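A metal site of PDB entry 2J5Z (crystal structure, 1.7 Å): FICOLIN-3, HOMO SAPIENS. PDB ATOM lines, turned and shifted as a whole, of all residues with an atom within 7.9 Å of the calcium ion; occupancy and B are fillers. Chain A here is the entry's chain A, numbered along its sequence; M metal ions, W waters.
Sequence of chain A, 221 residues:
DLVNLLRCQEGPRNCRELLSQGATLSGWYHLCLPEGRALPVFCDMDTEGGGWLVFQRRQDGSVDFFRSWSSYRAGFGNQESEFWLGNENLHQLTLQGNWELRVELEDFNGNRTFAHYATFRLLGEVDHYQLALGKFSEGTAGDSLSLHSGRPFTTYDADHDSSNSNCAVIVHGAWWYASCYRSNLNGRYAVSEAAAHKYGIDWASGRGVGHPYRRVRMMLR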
ATOM      1  N   THR A 154     -26.731  -3.826  -4.008  1.00  0.00           N
ATOM      2  CA  THR A 154     -25.337  -3.981  -3.546  1.00  0.00           C
ATOM      3  C   THR A 154     -24.415  -2.887  -4.063  1.00  0.00           C
ATOM      4  O   THR A 154     -24.558  -2.401  -5.205  1.00  0.00           O
ATOM      5  CB  THR A 154     -24.679  -5.419  -3.743  1.00  0.00           C
ATOM      6  OG1 THR A 154     -23.677  -5.425  -4.778  1.00  0.00           O
ATOM      7  CG2 THR A 154     -25.689  -6.470  -3.955  1.00  0.00           C
ATOM      8  N   ALA A 158     -20.976  -3.226   0.326  1.00  0.00           N
ATOM      9  CA  ALA A 158     -22.128  -3.954   0.856  1.00  0.00           C
ATOM     10  C   ALA A 158     -22.590  -5.012  -0.151  1.00  0.00           C
ATOM     11  O   ALA A 158     -23.498  -4.772  -0.950  1.00  0.00           O
ATOM     12  CB  ALA A 158     -23.256  -2.991   1.200  1.00  0.00           C
ATOM     13  N   ASP A 159     -21.936  -6.174  -0.094  1.00  0.00           N
ATOM     14  CA  ASP A 159     -22.199  -7.262  -1.041  1.00  0.00           C
ATOM     15  C   ASP A 159     -23.404  -8.097  -0.629  1.00  0.00           C
ATOM     16  O   ASP A 159     -23.368  -8.815   0.373  1.00  0.00           O
ATOM     17  CB  ASP A 159     -20.949  -8.139  -1.207  1.00  0.00           C
ATOM     18  CG  ASP A 159     -21.095  -9.206  -2.298  1.00  0.00           C
ATOM     19  OD1 ASP A 159     -22.220  -9.432  -2.817  1.00  0.00           O
ATOM     20  OD2 ASP A 159     -20.079  -9.856  -2.636  1.00  0.00           O
ATOM     21  N   HIS A 160     -24.478  -8.003  -1.411  1.00  0.00           N
ATOM     22  CA  HIS A 160     -25.705  -8.722  -1.108  1.00  0.00           C
ATOM     23  C   HIS A 160     -26.155  -9.563  -2.291  1.00  0.00           C
ATOM     24  O   HIS A 160     -27.265 -10.104  -2.286  1.00  0.00           O
ATOM     25  CB  HIS A 160     -26.836  -7.742  -0.755  1.00  0.00           C
ATOM     26  CG  HIS A 160     -26.506  -6.811   0.372  1.00  0.00           C
ATOM     27  ND1 HIS A 160     -26.225  -7.256   1.653  1.00  0.00           N
ATOM     28  CD2 HIS A 160     -26.426  -5.460   0.416  1.00  0.00           C
ATOM     29  CE1 HIS A 160     -25.988  -6.218   2.433  1.00  0.00           C
ATOM     30  NE2 HIS A 160     -26.098  -5.119   1.702  1.00  0.00           N
ATOM     31  N   ASP A 161     -25.313  -9.666  -3.311  1.00  0.00           N
ATOM     32  CA  ASP A 161     -25.743 -10.260  -4.575  1.00  0.00           C
ATOM     33  C   ASP A 161     -25.711 -11.793  -4.525  1.00  0.00           C
ATOM     34  O   ASP A 161     -25.536 -12.368  -3.461  1.00  0.00           O
ATOM     35  CB  ASP A 161     -24.930  -9.707  -5.758  1.00  0.00           C
ATOM     36  CG  ASP A 161     -23.448 -10.011  -5.643  1.00  0.00           C
ATOM     37  OD1 ASP A 161     -23.096 -11.117  -5.168  1.00  0.00           O
ATOM     38  OD2 ASP A 161     -22.639  -9.145  -6.040  1.00  0.00           O
ATOM     39  N   SER A 162     -25.925 -12.439  -5.663  1.00  0.00           N
ATOM     40  CA  SER A 162     -26.005 -13.897  -5.703  1.00  0.00           C
ATOM     41  C   SER A 162     -24.753 -14.485  -6.341  1.00  0.00           C
ATOM     42  O   SER A 162     -24.743 -15.628  -6.788  1.00  0.00           O
ATOM     43  CB  SER A 162     -27.250 -14.331  -6.473  1.00  0.00           C
ATOM     44  OG  SER A 162     -27.228 -13.877  -7.813  1.00  0.00           O
ATOM     45  N   SER A 163     -23.696 -13.678  -6.383  1.00  0.00           N
ATOM     46  CA  SER A 163     -22.429 -14.082  -6.992  1.00  0.00           C
ATOM     47  C   SER A 163     -21.399 -14.430  -5.916  1.00  0.00           C
ATOM     48  O   SER A 163     -21.462 -13.903  -4.806  1.00  0.00           O
ATOM     49  CB  SER A 163     -21.904 -12.932  -7.866  1.00  0.00           C
ATOM     50  OG  SER A 163     -20.613 -13.213  -8.375  1.00  0.00           O
ATOM     51  N   ASN A 164     -20.461 -15.317  -6.253  1.00  0.00           N
ATOM     52  CA  ASN A 164     -19.373 -15.669  -5.337  1.00  0.00           C
ATOM     53  C   ASN A 164     -18.435 -14.482  -5.185  1.00  0.00           C
ATOM     54  O   ASN A 164     -17.578 -14.456  -4.296  1.00  0.00           O
ATOM     55  CB  ASN A 164     -18.610 -16.899  -5.848  1.00  0.00           C
ATOM     56  N   SER A 165     -18.609 -13.502  -6.058  1.00  0.00           N
ATOM     57  CA  SER A 165     -17.862 -12.248  -5.986  1.00  0.00           C
ATOM     58  C   SER A 165     -18.762 -11.065  -5.605  1.00  0.00           C
ATOM     59  O   SER A 165     -19.958 -11.240  -5.308  1.00  0.00           O
ATOM     60  CB  SER A 165     -17.176 -11.970  -7.324  1.00  0.00           C
ATOM     61  OG  SER A 165     -18.116 -11.724  -8.353  1.00  0.00           O
ATOM     62  N   ASN A 166     -18.156  -9.880  -5.604  1.00  0.00           N
ATOM     63  CA  ASN A 166     -18.870  -8.620  -5.420  1.00  0.00           C
ATOM     64  C   ASN A 166     -19.110  -7.956  -6.767  1.00  0.00           C
ATOM     65  O   ASN A 166     -18.199  -7.332  -7.341  1.00  0.00           O
ATOM     66  CB  ASN A 166     -18.066  -7.691  -4.481  1.00  0.00           C
ATOM     67  CG  ASN A 166     -18.749  -6.360  -4.248  1.00  0.00           C
ATOM     68  OD1 ASN A 166     -19.306  -5.765  -5.167  1.00  0.00           O
ATOM     69  ND2 ASN A 166     -18.703  -5.873  -3.007  1.00  0.00           N
ATOM     70  N   CYS A 167     -20.332  -8.099  -7.283  1.00  0.00           N
ATOM     71  CA  CYS A 167     -20.675  -7.568  -8.594  1.00  0.00           C
ATOM     72  C   CYS A 167     -20.417  -6.070  -8.731  1.00  0.00           C
ATOM     73  O   CYS A 167     -20.051  -5.612  -9.795  1.00  0.00           O
ATOM     74  CB  CYS A 167     -22.147  -7.823  -8.911  1.00  0.00           C
ATOM     75  SG  CYS A 167     -22.506  -9.525  -9.378  1.00  0.00           S
ATOM     76  N   ALA A 168     -20.681  -5.313  -7.663  1.00  0.00           N
ATOM     77  CA  ALA A 168     -20.450  -3.870  -7.691  1.00  0.00           C
ATOM     78  C   ALA A 168     -18.974  -3.593  -7.969  1.00  0.00           C
ATOM     79  O   ALA A 168     -18.636  -2.750  -8.797  1.00  0.00           O
ATOM     80  CB  ALA A 168     -20.883  -3.228  -6.393  1.00  0.00           C
ATOM     81  N   ALA A 178     -27.564  -9.512  -9.594  1.00  0.00           N
ATOM     82  CA  ALA A 178     -27.683 -10.948  -9.459  1.00  0.00           C
ATOM     83  C   ALA A 178     -26.261 -11.511  -9.628  1.00  0.00           C
ATOM     84  O   ALA A 178     -25.467 -11.491  -8.687  1.00  0.00           O
ATOM     85  CB  ALA A 178     -28.632 -11.488 -10.518  1.00  0.00           C
ATOM     86  N   SER A 179     -25.927 -12.000 -10.817  1.00  0.00           N
ATOM     87  CA  SER A 179     -24.554 -12.427 -11.100  1.00  0.00           C
ATOM     88  C   SER A 179     -24.164 -12.309 -12.586  1.00  0.00           C
ATOM     89  O   SER A 179     -23.895 -13.312 -13.255  1.00  0.00           O
ATOM     90  CB  SER A 179     -24.311 -13.845 -10.561  1.00  0.00           C
ATOM     91  OG  SER A 179     -25.365 -14.721 -10.915  1.00  0.00           O
HETATM   92 CA    CA M   1     -21.427 -11.709  -3.628  1.00  0.00          CA
HETATM   93  O   HOH W   1     -23.084 -12.640  -2.223  1.00  0.00           O
HETATM   94  O   HOH W   2     -19.966 -12.907  -2.114  1.00  0.00           O
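The calcium ion is bound by the backbone carbonyl oxygen (O) of Ser 165, the side-chain carboxylate (OD1) of Asp 161, water W1, water W2, the backbone carbonyl oxygen (O) of Ser 163, the side-chain carboxylate (OD2) of Asp 159 and the side-chain carboxylate (OD1) of Asp 159. The calcium ion has seven donor atoms within binding distance.
The nearest printed residue that does not touch the calcium ion is Asn 166 (4.2 Å).
The backbone NH (N) of Cys 167 sits at hydrogen-bond distance from the side-chain carboxylate (OD2) of Asp 161, at 2.8 Å. The side-chain hydroxyl (OG) of Ser 165 sits at hydrogen-bond distance from the side-chain hydroxyl (OG) of Ser 163 (2.9 Å).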
